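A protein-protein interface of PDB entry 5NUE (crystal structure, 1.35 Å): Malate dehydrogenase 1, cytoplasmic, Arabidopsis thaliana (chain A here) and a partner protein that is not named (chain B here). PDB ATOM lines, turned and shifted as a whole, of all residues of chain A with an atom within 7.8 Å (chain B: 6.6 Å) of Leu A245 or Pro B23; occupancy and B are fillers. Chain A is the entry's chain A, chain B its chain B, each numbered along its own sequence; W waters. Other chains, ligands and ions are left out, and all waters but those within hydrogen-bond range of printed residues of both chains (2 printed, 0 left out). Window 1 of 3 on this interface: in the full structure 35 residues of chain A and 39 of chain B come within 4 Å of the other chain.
The side-chain carboxylate (OE1) of Glu B57 sits at hydrogen-bond distance from the backbone NH (N) of Leu A245 (3.3 Å). NH1 of Arg A239 lies within hydrogen-bond range of OH of Tyr B19 (3.4 Å). The side-chain hydroxyl (OH) of Tyr B19 is in hydrogen-bond range of the backbone NH (N) of Ala A244, 3.3 Å away. The side-chain hydroxyl (OG) of Ser A246 lies within hydrogen-bond range of the side-chain carboxylate (OE1) of Glu B57 (2.7 Å). NH2 of Arg B27 sits at hydrogen-bond distance from OG of Ser A249 (2.7 Å). The backbone NH (N) of Ala A244 lies within hydrogen-bond range of the side-chain carboxylate (OE1) of Glu B57, 3.0 Å away. OH of Tyr B19 sits at hydrogen-bond distance from N of Leu A245, 2.8 Å away. OE2 of Glu B57 is in salt-bridge range of NH1 of Arg A239 (3.0 Å).
Water W2 lies within hydrogen-bond range of OG of Ser A249 (2.6 Å), O of Ala B61 (2.7 Å) and N of Ser A250 (3.4 Å). Water W1 lies within hydrogen-bond range of NE of Arg B27 (2.8 Å), OG of Ser A249 (3.0 Å) and SD of Met A24 (3.3 Å).
Of the 21 printed residues of chain A, 8 touch a printed residue of chain B. Hydrophobic or aromatic side chains of chain A within 4 Å of the printed part of chain B: Ile A29, Ile A235, Ala A244 and Leu A245. Hydrophobic or aromatic side chains of chain B within 4 Å of the printed part of chain A: Tyr B19, Val B22, Pro B23 and Phe B63. Among the printed residues, 14 pairs touch across the chains. Among the printed residues, Asp or Glu carboxylates within 4 Å of a Lys or Arg side-chain nitrogen of the other chain: Arg A239 with Glu B57 (3.0 Å).
The backbone carbonyl oxygen (O) of Ser A246 is in hydrogen-bond range of the side-chain hydroxyl (OG) of Ser A250, at 2.9 Å. O of Met A24 lies within hydrogen-bond range of N of Ile A29, 3.0 Å away. SD of Met A24 lies within hydrogen-bond range of N of Ser A249 (3.7 Å). The side-chain hydroxyl of Tyr B19 lies within hydrogen-bond range of the side-chain carboxylate of Glu B57 (2.6 Å). The side-chain amide oxygen (OE1) of Gln A16 sits at hydrogen-bond distance from the guanidinium group (NH2) of Arg A239 (2.7 Å). The guanidinium group of Arg A239 lies within hydrogen-bond range of the backbone carbonyl oxygen of Ser A242 (3.1 Å).
Arg B27 touches Ile A29 (NE to CG2, 3.4 Å). CG of Glu B57 touches CD1 of Ile A235 (3.9 Å). OE1 of Glu B57 touches CA of Ser A243 (3.5 Å). Leu A245 touches Val B22. CG of Leu A245 touches CB of Pro B23, at 3.9 Å. Phe B63 touches Ser A249.
Of the printed residues of chain B, Arg A239 touches Tyr B19 (3.4 Å) and Glu B57 (3.0 Å). Of the printed residues of chain B, Ser A243 touches Glu B57 (3.5 Å). Of the printed residues of chain B, Leu A245 touches Tyr B19 (2.8 Å), Val B22 (3.9 Å), Pro B23 (3.9 Å) and Glu B57 (3.3 Å). Printed residues of chain B within 4 Å of Ser A246: Glu B57 (2.7 Å). Ser A250 touches none of the printed residues of chain B. Of the printed residues of chain A, Tyr B19 touches Arg A239, Ala A244 and Leu A245. Of the printed residues of chain A, Pro B23 touches Leu A245. Gly B28 touches none of the printed residues of chain A. The nearest residue of chain B that does not touch Leu A245 is Val B54 (4.2 Å). The nearest printed residue of chain A that does not touch Tyr B19 is Gln A16 (4.04 Å).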
ATOM      1  N   GLN A  16     -20.854 -35.333   3.651  1.00  0.00           N
ATOM      2  CA  GLN A  16     -21.897 -34.332   3.427  1.00  0.00           C
ATOM      3  C   GLN A  16     -21.460 -33.241   2.440  1.00  0.00           C
ATOM      4  O   GLN A  16     -22.183 -32.912   1.479  1.00  0.00           O
ATOM      5  CB  GLN A  16     -22.268 -33.717   4.767  1.00  0.00           C
ATOM      6  CG  GLN A  16     -23.598 -32.993   4.672  1.00  0.00           C
ATOM      7  CD  GLN A  16     -23.938 -32.021   5.855  1.00  0.00           C
ATOM      8  OE1 GLN A  16     -25.076 -31.535   5.909  1.00  0.00           O
ATOM      9  NE2 GLN A  16     -22.945 -31.707   6.742  1.00  0.00           N
ATOM     10  N   ILE A  17     -20.312 -32.616   2.701  1.00  0.00           N
ATOM     11  CA  ILE A  17     -19.806 -31.586   1.789  1.00  0.00           C
ATOM     12  C   ILE A  17     -19.474 -32.183   0.428  1.00  0.00           C
ATOM     13  O   ILE A  17     -19.795 -31.594  -0.613  1.00  0.00           O
ATOM     14  CB  ILE A  17     -18.610 -30.840   2.401  1.00  0.00           C
ATOM     15  CG1 ILE A  17     -19.073 -29.937   3.569  1.00  0.00           C
ATOM     16  CG2 ILE A  17     -17.949 -29.974   1.344  1.00  0.00           C
ATOM     17  CD1 ILE A  17     -17.904 -29.273   4.336  1.00  0.00           C
ATOM     18  N   ALA A  20     -22.570 -32.494  -1.681  1.00  0.00           N
ATOM     19  CA  ALA A  20     -23.021 -31.196  -2.168  1.00  0.00           C
ATOM     20  C   ALA A  20     -22.078 -30.618  -3.215  1.00  0.00           C
ATOM     21  O   ALA A  20     -22.503 -29.838  -4.084  1.00  0.00           O
ATOM     22  CB  ALA A  20     -23.103 -30.224  -0.988  1.00  0.00           C
ATOM     23  N   LEU A  21     -20.797 -30.975  -3.151  1.00  0.00           N
ATOM     24  CA  LEU A  21     -19.785 -30.315  -3.970  1.00  0.00           C
ATOM     25  C   LEU A  21     -19.607 -30.983  -5.324  1.00  0.00           C
ATOM     26  O   LEU A  21     -19.469 -30.292  -6.340  1.00  0.00           O
ATOM     27  CB  LEU A  21     -18.410 -30.348  -3.264  1.00  0.00           C
ATOM     28  CG  LEU A  21     -17.222 -29.744  -4.005  1.00  0.00           C
ATOM     29  CD1 LEU A  21     -17.422 -28.286  -4.409  1.00  0.00           C
ATOM     30  CD2 LEU A  21     -15.949 -29.891  -3.088  1.00  0.00           C
ATOM     31  N   PRO A  23     -21.551 -32.400  -7.570  1.00  0.00           N
ATOM     32  CA  PRO A  23     -22.404 -31.985  -8.697  1.00  0.00           C
ATOM     33  C   PRO A  23     -22.145 -30.547  -9.099  1.00  0.00           C
ATOM     34  O   PRO A  23     -22.369 -30.191 -10.271  1.00  0.00           O
ATOM     35  CB  PRO A  23     -23.830 -32.195  -8.172  1.00  0.00           C
ATOM     36  CG  PRO A  23     -23.711 -31.980  -6.650  1.00  0.00           C
ATOM     37  CD  PRO A  23     -22.335 -32.566  -6.320  1.00  0.00           C
ATOM     38  N   MET A  24     -21.694 -29.693  -8.172  1.00  0.00           N
ATOM     39  CA  MET A  24     -21.346 -28.313  -8.534  1.00  0.00           C
ATOM     40  C   MET A  24     -20.148 -28.289  -9.472  1.00  0.00           C
ATOM     41  O   MET A  24     -20.150 -27.571 -10.477  1.00  0.00           O
ATOM     42  CB  MET A  24     -21.044 -27.480  -7.283  1.00  0.00           C
ATOM     43  CG  MET A  24     -22.213 -27.393  -6.284  1.00  0.00           C
ATOM     44  SD  MET A  24     -21.687 -26.316  -4.908  1.00  0.00           S
ATOM     45  CE  MET A  24     -23.102 -26.436  -3.815  1.00  0.00           C
ATOM     46  N   ILE A  29     -19.614 -25.118 -12.150  1.00  0.00           N
ATOM     47  CA  ILE A  29     -19.648 -23.980 -11.239  1.00  0.00           C
ATOM     48  C   ILE A  29     -18.259 -23.633 -10.723  1.00  0.00           C
ATOM     49  O   ILE A  29     -17.995 -22.479 -10.343  1.00  0.00           O
ATOM     50  CB  ILE A  29     -20.667 -24.265 -10.124  1.00  0.00           C
ATOM     51  CG1 ILE A  29     -22.003 -24.619 -10.774  1.00  0.00           C
ATOM     52  CG2 ILE A  29     -20.811 -23.058  -9.170  1.00  0.00           C
ATOM     53  CD1 ILE A  29     -23.088 -25.029  -9.811  1.00  0.00           C
ATOM     54  N   LEU A 159     -16.196 -19.281   3.043  1.00  0.00           N
ATOM     55  CA  LEU A 159     -17.518 -19.359   3.655  1.00  0.00           C
ATOM     56  C   LEU A 159     -17.673 -18.300   4.728  1.00  0.00           C
ATOM     57  O   LEU A 159     -18.709 -17.663   4.814  1.00  0.00           O
ATOM     58  CB  LEU A 159     -17.820 -20.762   4.202  1.00  0.00           C
ATOM     59  CG  LEU A 159     -19.158 -20.894   4.942  1.00  0.00           C
ATOM     60  CD1 LEU A 159     -20.376 -20.459   4.034  1.00  0.00           C
ATOM     61  CD2 LEU A 159     -19.361 -22.340   5.440  1.00  0.00           C
ATOM     62  N   ILE A 235     -25.499 -22.956  12.457  1.00  0.00           N
ATOM     63  CA  ILE A 235     -25.986 -23.929  11.482  1.00  0.00           C
ATOM     64  C   ILE A 235     -26.153 -25.283  12.157  1.00  0.00           C
ATOM     65  O   ILE A 235     -27.160 -25.962  11.961  1.00  0.00           O
ATOM     66  CB  ILE A 235     -25.037 -24.040  10.269  1.00  0.00           C
ATOM     67  CG1 ILE A 235     -24.870 -22.695   9.530  1.00  0.00           C
ATOM     68  CG2 ILE A 235     -25.521 -25.141   9.274  1.00  0.00           C
ATOM     69  CD1 ILE A 235     -26.137 -22.073   9.019  1.00  0.00           C
ATOM     70  N   ARG A 239     -29.575 -27.400  12.088  1.00  0.00           N
ATOM     71  CA  ARG A 239     -29.698 -28.575  11.244  1.00  0.00           C
ATOM     72  C   ARG A 239     -29.224 -29.861  11.892  1.00  0.00           C
ATOM     73  O   ARG A 239     -29.467 -30.939  11.319  1.00  0.00           O
ATOM     74  CB  ARG A 239     -28.871 -28.373   9.967  1.00  0.00           C
ATOM     75  CG  ARG A 239     -29.437 -27.278   9.085  1.00  0.00           C
ATOM     76  CD  ARG A 239     -28.661 -27.098   7.766  1.00  0.00           C
ATOM     77  NE  ARG A 239     -28.561 -28.397   7.135  1.00  0.00           N
ATOM     78  CZ  ARG A 239     -27.409 -29.067   6.994  1.00  0.00           C
ATOM     79  NH1 ARG A 239     -26.269 -28.501   7.329  1.00  0.00           N
ATOM     80  NH2 ARG A 239     -27.405 -30.287   6.535  1.00  0.00           N
ATOM     81  N   SER A 242     -23.134 -29.690  10.567  1.00  0.00           N
ATOM     82  CA  SER A 242     -22.459 -28.479  10.123  1.00  0.00           C
ATOM     83  C   SER A 242     -22.753 -28.186   8.634  1.00  0.00           C
ATOM     84  O   SER A 242     -23.310 -29.007   7.892  1.00  0.00           O
ATOM     85  CB  SER A 242     -20.970 -28.550  10.463  1.00  0.00           C
ATOM     86  OG  SER A 242     -20.374 -29.782  10.047  1.00  0.00           O
ATOM     87  N   SER A 243     -22.306 -27.010   8.199  1.00  0.00           N
ATOM     88  CA  SER A 243     -22.633 -26.500   6.871  1.00  0.00           C
ATOM     89  C   SER A 243     -22.125 -27.427   5.766  1.00  0.00           C
ATOM     90  O   SER A 243     -21.068 -28.067   5.882  1.00  0.00           O
ATOM     91  CB  SER A 243     -22.000 -25.119   6.676  1.00  0.00           C
ATOM     92  OG  SER A 243     -20.588 -25.186   6.713  1.00  0.00           O
ATOM     93  N   ALA A 244     -22.892 -27.498   4.683  1.00  0.00           N
ATOM     94  CA  ALA A 244     -22.447 -28.307   3.547  1.00  0.00           C
ATOM     95  C   ALA A 244     -22.808 -27.637   2.219  1.00  0.00           C
ATOM     96  O   ALA A 244     -21.923 -27.390   1.395  1.00  0.00           O
ATOM     97  CB  ALA A 244     -23.027 -29.727   3.640  1.00  0.00           C
ATOM     98  N   LEU A 245     -24.078 -27.278   2.027  1.00  0.00           N
ATOM     99  CA  LEU A 245     -24.472 -26.564   0.825  1.00  0.00           C
ATOM    100  C   LEU A 245     -23.604 -25.309   0.668  1.00  0.00           C
ATOM    101  O   LEU A 245     -23.063 -25.022  -0.413  1.00  0.00           O
ATOM    102  CB  LEU A 245     -25.970 -26.214   0.993  1.00  0.00           C
ATOM    103  CG  LEU A 245     -26.792 -25.246   0.202  1.00  0.00           C
ATOM    104  CD1 LEU A 245     -28.231 -25.379   0.735  1.00  0.00           C
ATOM    105  CD2 LEU A 245     -26.248 -23.843   0.181  1.00  0.00           C
ATOM    106  N   SER A 246     -23.490 -24.527   1.757  1.00  0.00           N
ATOM    107  CA  SER A 246     -22.760 -23.272   1.677  1.00  0.00           C
ATOM    108  C   SER A 246     -21.248 -23.472   1.700  1.00  0.00           C
ATOM    109  O   SER A 246     -20.518 -22.655   1.131  1.00  0.00           O
ATOM    110  CB  SER A 246     -23.212 -22.326   2.813  1.00  0.00           C
ATOM    111  OG  SER A 246     -23.087 -22.958   4.081  1.00  0.00           O
ATOM    112  N   ALA A 247     -20.742 -24.513   2.372  1.00  0.00           N
ATOM    113  CA  ALA A 247     -19.310 -24.811   2.303  1.00  0.00           C
ATOM    114  C   ALA A 247     -18.924 -25.227   0.877  1.00  0.00           C
ATOM    115  O   ALA A 247     -17.914 -24.746   0.359  1.00  0.00           O
ATOM    116  CB  ALA A 247     -18.979 -25.927   3.322  1.00  0.00           C
ATOM    117  N   ALA A 248     -19.709 -26.124   0.252  1.00  0.00           N
ATOM    118  CA  ALA A 248     -19.417 -26.561  -1.129  1.00  0.00           C
ATOM    119  C   ALA A 248     -19.471 -25.383  -2.083  1.00  0.00           C
ATOM    120  O   ALA A 248     -18.587 -25.210  -2.921  1.00  0.00           O
ATOM    121  CB  ALA A 248     -20.427 -27.630  -1.575  1.00  0.00           C
ATOM    122  N   SER A 249     -20.492 -24.524  -1.938  1.00  0.00           N
ATOM    123  CA  SER A 249     -20.606 -23.395  -2.853  1.00  0.00           C
ATOM    124  C   SER A 249     -19.427 -22.445  -2.672  1.00  0.00           C
ATOM    125  O   SER A 249     -18.893 -21.903  -3.647  1.00  0.00           O
ATOM    126  CB  SER A 249     -21.914 -22.663  -2.567  1.00  0.00           C
ATOM    127  OG  SER A 249     -22.110 -21.626  -3.523  1.00  0.00           O
ATOM    128  N   SER A 250     -19.022 -22.209  -1.414  1.00  0.00           N
ATOM    129  CA  SER A 250     -17.916 -21.288  -1.174  1.00  0.00           C
ATOM    130  C   SER A 250     -16.591 -21.876  -1.630  1.00  0.00           C
ATOM    131  O   SER A 250     -15.701 -21.130  -2.023  1.00  0.00           O
ATOM    132  CB  SER A 250     -17.865 -20.994   0.340  1.00  0.00           C
ATOM    133  OG  SER A 250     -19.015 -20.213   0.739  1.00  0.00           O
ATOM    134  N   ALA A 251     -16.441 -23.213  -1.569  1.00  0.00           N
ATOM    135  CA  ALA A 251     -15.234 -23.850  -2.111  1.00  0.00           C
ATOM    136  C   ALA A 251     -15.180 -23.648  -3.623  1.00  0.00           C
ATOM    137  O   ALA A 251     -14.103 -23.399  -4.198  1.00  0.00           O
ATOM    138  CB  ALA A 251     -15.254 -25.344  -1.774  1.00  0.00           C
ATOM    139  N   CYS A 252     -16.338 -23.761  -4.290  1.00  0.00           N
ATOM    140  CA  CYS A 252     -16.381 -23.439  -5.726  1.00  0.00           C
ATOM    141  C   CYS A 252     -15.952 -22.002  -5.981  1.00  0.00           C
ATOM    142  O   CYS A 252     -15.172 -21.734  -6.901  1.00  0.00           O
ATOM    143  CB  CYS A 252     -17.769 -23.687  -6.305  1.00  0.00           C
ATOM    144  SG  CYS A 252     -18.222 -25.410  -6.481  1.00  0.00           S
ATOM    145  N   ILE B  17     -33.505 -34.056  -1.184  1.00  0.00           N
ATOM    146  CA  ILE B  17     -33.548 -33.475  -2.532  1.00  0.00           C
ATOM    147  C   ILE B  17     -33.598 -31.956  -2.469  1.00  0.00           C
ATOM    148  O   ILE B  17     -32.893 -31.261  -3.224  1.00  0.00           O
ATOM    149  CB  ILE B  17     -34.698 -34.051  -3.358  1.00  0.00           C
ATOM    150  CG1 ILE B  17     -34.353 -35.519  -3.655  1.00  0.00           C
ATOM    151  CG2 ILE B  17     -34.863 -33.270  -4.670  1.00  0.00           C
ATOM    152  CD1 ILE B  17     -35.527 -36.224  -4.338  1.00  0.00           C
ATOM    153  N   GLY B  18     -34.415 -31.409  -1.555  1.00  0.00           N
ATOM    154  CA  GLY B  18     -34.476 -29.951  -1.429  1.00  0.00           C
ATOM    155  C   GLY B  18     -33.108 -29.355  -1.170  1.00  0.00           C
ATOM    156  O   GLY B  18     -32.740 -28.329  -1.758  1.00  0.00           O
ATOM    157  N   TYR B  19     -32.334 -29.989  -0.271  1.00  0.00           N
ATOM    158  CA  TYR B  19     -31.028 -29.462   0.094  1.00  0.00           C
ATOM    159  C   TYR B  19     -30.065 -29.510  -1.098  1.00  0.00           C
ATOM    160  O   TYR B  19     -29.211 -28.614  -1.258  1.00  0.00           O
ATOM    161  CB  TYR B  19     -30.488 -30.300   1.254  1.00  0.00           C
ATOM    162  CG  TYR B  19     -29.284 -29.703   1.948  1.00  0.00           C
ATOM    163  CD1 TYR B  19     -29.437 -28.640   2.865  1.00  0.00           C
ATOM    164  CD2 TYR B  19     -28.005 -30.249   1.780  1.00  0.00           C
ATOM    165  CE1 TYR B  19     -28.323 -28.081   3.501  1.00  0.00           C
ATOM    166  CE2 TYR B  19     -26.914 -29.728   2.431  1.00  0.00           C
ATOM    167  CZ  TYR B  19     -27.098 -28.669   3.323  1.00  0.00           C
ATOM    168  OH  TYR B  19     -26.002 -28.152   3.913  1.00  0.00           O
ATOM    169  N   ALA B  20     -30.173 -30.557  -1.930  1.00  0.00           N
ATOM    170  CA  ALA B  20     -29.373 -30.657  -3.152  1.00  0.00           C
ATOM    171  C   ALA B  20     -29.846 -29.683  -4.231  1.00  0.00           C
ATOM    172  O   ALA B  20     -29.038 -29.239  -5.081  1.00  0.00           O
ATOM    173  CB  ALA B  20     -29.465 -32.093  -3.686  1.00  0.00           C
ATOM    174  N   LEU B  21     -31.140 -29.328  -4.217  1.00  0.00           N
ATOM    175  CA  LEU B  21     -31.753 -28.584  -5.335  1.00  0.00           C
ATOM    176  C   LEU B  21     -31.641 -27.079  -5.150  1.00  0.00           C
ATOM    177  O   LEU B  21     -31.312 -26.362  -6.108  1.00  0.00           O
ATOM    178  CB  LEU B  21     -33.214 -28.991  -5.451  1.00  0.00           C
ATOM    179  CG  LEU B  21     -34.001 -28.203  -6.531  1.00  0.00           C
ATOM    180  CD1 LEU B  21     -33.360 -28.391  -7.922  1.00  0.00           C
ATOM    181  CD2 LEU B  21     -35.415 -28.729  -6.573  1.00  0.00           C
ATOM    182  N   VAL B  22     -31.918 -26.552  -3.950  1.00  0.00           N
ATOM    183  CA  VAL B  22     -31.919 -25.087  -3.796  1.00  0.00           C
ATOM    184  C   VAL B  22     -30.626 -24.393  -4.176  1.00  0.00           C
ATOM    185  O   VAL B  22     -30.690 -23.312  -4.784  1.00  0.00           O
ATOM    186  CB  VAL B  22     -32.504 -24.656  -2.437  1.00  0.00           C
ATOM    187  CG1 VAL B  22     -33.976 -25.143  -2.335  1.00  0.00           C
ATOM    188  CG2 VAL B  22     -31.627 -25.160  -1.261  1.00  0.00           C
ATOM    189  N   PRO B  23     -29.434 -24.929  -3.907  1.00  0.00           N
ATOM    190  CA  PRO B  23     -28.258 -24.176  -4.362  1.00  0.00           C
ATOM    191  C   PRO B  23     -28.129 -24.198  -5.869  1.00  0.00           C
ATOM    192  O   PRO B  23     -27.527 -23.275  -6.445  1.00  0.00           O
ATOM    193  CB  PRO B  23     -27.071 -24.915  -3.697  1.00  0.00           C
ATOM    194  CG  PRO B  23     -27.547 -26.320  -3.500  1.00  0.00           C
ATOM    195  CD  PRO B  23     -29.052 -26.164  -3.177  1.00  0.00           C
ATOM    196  N   MET B  24     -28.592 -25.266  -6.529  1.00  0.00           N
ATOM    197  CA  MET B  24     -28.538 -25.298  -7.992  1.00  0.00           C
ATOM    198  C   MET B  24     -29.421 -24.208  -8.579  1.00  0.00           C
ATOM    199  O   MET B  24     -29.026 -23.520  -9.532  1.00  0.00           O
ATOM    200  CB  MET B  24     -29.034 -26.656  -8.503  1.00  0.00           C
ATOM    201  CG  MET B  24     -28.242 -27.851  -8.003  1.00  0.00           C
ATOM    202  SD  MET B  24     -28.926 -29.368  -8.719  1.00  0.00           S
ATOM    203  CE  MET B  24     -27.862 -30.574  -7.961  1.00  0.00           C
ATOM    204  N   ILE B  25     -30.623 -24.027  -8.004  1.00  0.00           N
ATOM    205  CA  ILE B  25     -31.495 -22.943  -8.437  1.00  0.00           C
ATOM    206  C   ILE B  25     -30.815 -21.602  -8.208  1.00  0.00           C
ATOM    207  O   ILE B  25     -30.795 -20.742  -9.107  1.00  0.00           O
ATOM    208  CB  ILE B  25     -32.858 -23.020  -7.734  1.00  0.00           C
ATOM    209  CG1 ILE B  25     -33.583 -24.330  -8.086  1.00  0.00           C
ATOM    210  CG2 ILE B  25     -33.723 -21.827  -8.174  1.00  0.00           C
ATOM    211  CD1 ILE B  25     -34.808 -24.646  -7.230  1.00  0.00           C
ATOM    212  N   ALA B  26     -30.243 -21.402  -7.007  1.00  0.00           N
ATOM    213  CA  ALA B  26     -29.630 -20.125  -6.674  1.00  0.00           C
ATOM    214  C   ALA B  26     -28.446 -19.786  -7.568  1.00  0.00           C
ATOM    215  O   ALA B  26     -28.139 -18.604  -7.774  1.00  0.00           O
ATOM    216  CB  ALA B  26     -29.235 -20.080  -5.193  1.00  0.00           C
ATOM    217  N   ARG B  27     -27.745 -20.796  -8.055  1.00  0.00           N
ATOM    218  CA  ARG B  27     -26.572 -20.589  -8.892  1.00  0.00           C
ATOM    219  C   ARG B  27     -26.927 -20.362 -10.355  1.00  0.00           C
ATOM    220  O   ARG B  27     -26.028 -20.084 -11.152  1.00  0.00           O
ATOM    221  CB  ARG B  27     -25.680 -21.831  -8.755  1.00  0.00           C
ATOM    222  CG  ARG B  27     -24.293 -21.620  -9.253  1.00  0.00           C
ATOM    223  CD  ARG B  27     -23.630 -20.489  -8.492  1.00  0.00           C
ATOM    224  NE  ARG B  27     -22.802 -20.916  -7.376  1.00  0.00           N
ATOM    225  CZ  ARG B  27     -21.923 -20.095  -6.819  1.00  0.00           C
ATOM    226  NH1 ARG B  27     -21.864 -18.832  -7.261  1.00  0.00           N
ATOM    227  NH2 ARG B  27     -21.136 -20.510  -5.825  1.00  0.00           N
ATOM    228  N   GLY B  28     -28.199 -20.478 -10.734  1.00  0.00           N
ATOM    229  CA  GLY B  28     -28.602 -20.249 -12.120  1.00  0.00           C
ATOM    230  C   GLY B  28     -28.710 -21.491 -12.982  1.00  0.00           C
ATOM    231  O   GLY B  28     -28.884 -21.368 -14.206  1.00  0.00           O
ATOM    232  N   ILE B  29     -28.613 -22.694 -12.390  1.00  0.00           N
ATOM    233  CA  ILE B  29     -28.592 -23.907 -13.199  1.00  0.00           C
ATOM    234  C   ILE B  29     -29.974 -24.237 -13.738  1.00  0.00           C
ATOM    235  O   ILE B  29     -30.100 -24.897 -14.775  1.00  0.00           O
ATOM    236  CB  ILE B  29     -28.011 -25.063 -12.363  1.00  0.00           C
ATOM    237  CG1 ILE B  29     -26.648 -24.636 -11.805  1.00  0.00           C
ATOM    238  CG2 ILE B  29     -27.958 -26.379 -13.172  1.00  0.00           C
ATOM    239  CD1 ILE B  29     -25.599 -24.333 -12.868  1.00  0.00           C
ATOM    240  N   LEU B  39     -36.267 -17.549  -4.068  1.00  0.00           N
ATOM    241  CA  LEU B  39     -36.696 -18.885  -3.663  1.00  0.00           C
ATOM    242  C   LEU B  39     -37.791 -18.798  -2.615  1.00  0.00           C
ATOM    243  O   LEU B  39     -37.717 -17.992  -1.682  1.00  0.00           O
ATOM    244  CB  LEU B  39     -35.523 -19.657  -3.042  1.00  0.00           C
ATOM    245  CG  LEU B  39     -34.602 -20.372  -4.009  1.00  0.00           C
ATOM    246  CD1 LEU B  39     -33.314 -20.788  -3.228  1.00  0.00           C
ATOM    247  CD2 LEU B  39     -35.314 -21.599  -4.549  1.00  0.00           C
ATOM    248  N   VAL B  54     -31.538 -24.260   6.372  1.00  0.00           N
ATOM    249  CA  VAL B  54     -31.273 -24.234   4.935  1.00  0.00           C
ATOM    250  C   VAL B  54     -31.267 -22.793   4.430  1.00  0.00           C
ATOM    251  O   VAL B  54     -30.398 -22.393   3.636  1.00  0.00           O
ATOM    252  CB  VAL B  54     -32.284 -25.110   4.172  1.00  0.00           C
ATOM    253  CG1 VAL B  54     -31.965 -25.044   2.625  1.00  0.00           C
ATOM    254  CG2 VAL B  54     -32.237 -26.549   4.672  1.00  0.00           C
ATOM    255  N   GLU B  57     -28.037 -21.160   5.305  1.00  0.00           N
ATOM    256  CA  GLU B  57     -26.935 -21.535   4.401  1.00  0.00           C
ATOM    257  C   GLU B  57     -27.058 -20.877   3.022  1.00  0.00           C
ATOM    258  O   GLU B  57     -26.028 -20.507   2.447  1.00  0.00           O
ATOM    259  CB  GLU B  57     -26.847 -23.033   4.215  1.00  0.00           C
ATOM    260  CG  GLU B  57     -26.328 -23.759   5.475  1.00  0.00           C
ATOM    261  CD  GLU B  57     -25.734 -25.099   5.119  1.00  0.00           C
ATOM    262  OE1 GLU B  57     -24.692 -25.148   4.427  1.00  0.00           O
ATOM    263  OE2 GLU B  57     -26.320 -26.112   5.508  1.00  0.00           O
ATOM    264  N   LEU B  58     -28.297 -20.684   2.521  1.00  0.00           N
ATOM    265  CA  LEU B  58     -28.445 -19.983   1.242  1.00  0.00           C
ATOM    266  C   LEU B  58     -27.953 -18.563   1.366  1.00  0.00           C
ATOM    267  O   LEU B  58     -27.284 -18.058   0.470  1.00  0.00           O
ATOM    268  CB  LEU B  58     -29.911 -19.979   0.804  1.00  0.00           C
ATOM    269  CG  LEU B  58     -30.360 -21.368   0.277  1.00  0.00           C
ATOM    270  CD1 LEU B  58     -31.868 -21.349   0.212  1.00  0.00           C
ATOM    271  CD2 LEU B  58     -29.787 -21.663  -1.109  1.00  0.00           C
ATOM    272  N   ALA B  61     -24.105 -18.412   1.482  1.00  0.00           N
ATOM    273  CA  ALA B  61     -23.379 -18.690   0.253  1.00  0.00           C
ATOM    274  C   ALA B  61     -23.215 -17.448  -0.617  1.00  0.00           C
ATOM    275  O   ALA B  61     -22.459 -17.504  -1.594  1.00  0.00           O
ATOM    276  CB  ALA B  61     -24.156 -19.751  -0.513  1.00  0.00           C
ATOM    277  N   PHE B  63     -25.084 -15.978  -2.929  1.00  0.00           N
ATOM    278  CA  PHE B  63     -25.384 -16.244  -4.341  1.00  0.00           C
ATOM    279  C   PHE B  63     -25.821 -14.965  -5.060  1.00  0.00           C
ATOM    280  O   PHE B  63     -26.875 -14.404  -4.733  1.00  0.00           O
ATOM    281  CB  PHE B  63     -26.544 -17.229  -4.440  1.00  0.00           C
ATOM    282  CG  PHE B  63     -26.201 -18.642  -4.085  1.00  0.00           C
ATOM    283  CD1 PHE B  63     -25.342 -19.414  -4.891  1.00  0.00           C
ATOM    284  CD2 PHE B  63     -26.773 -19.215  -2.953  1.00  0.00           C
ATOM    285  CE1 PHE B  63     -25.086 -20.728  -4.575  1.00  0.00           C
ATOM    286  CE2 PHE B  63     -26.489 -20.530  -2.601  1.00  0.00           C
ATOM    287  CZ  PHE B  63     -25.646 -21.304  -3.431  1.00  0.00           C
HETATM  288  O   HOH W   1     -22.688 -23.330  -5.929  1.00  0.00           O
HETATM  289  O   HOH W   2     -20.952 -19.609  -2.301  1.00  0.00           O
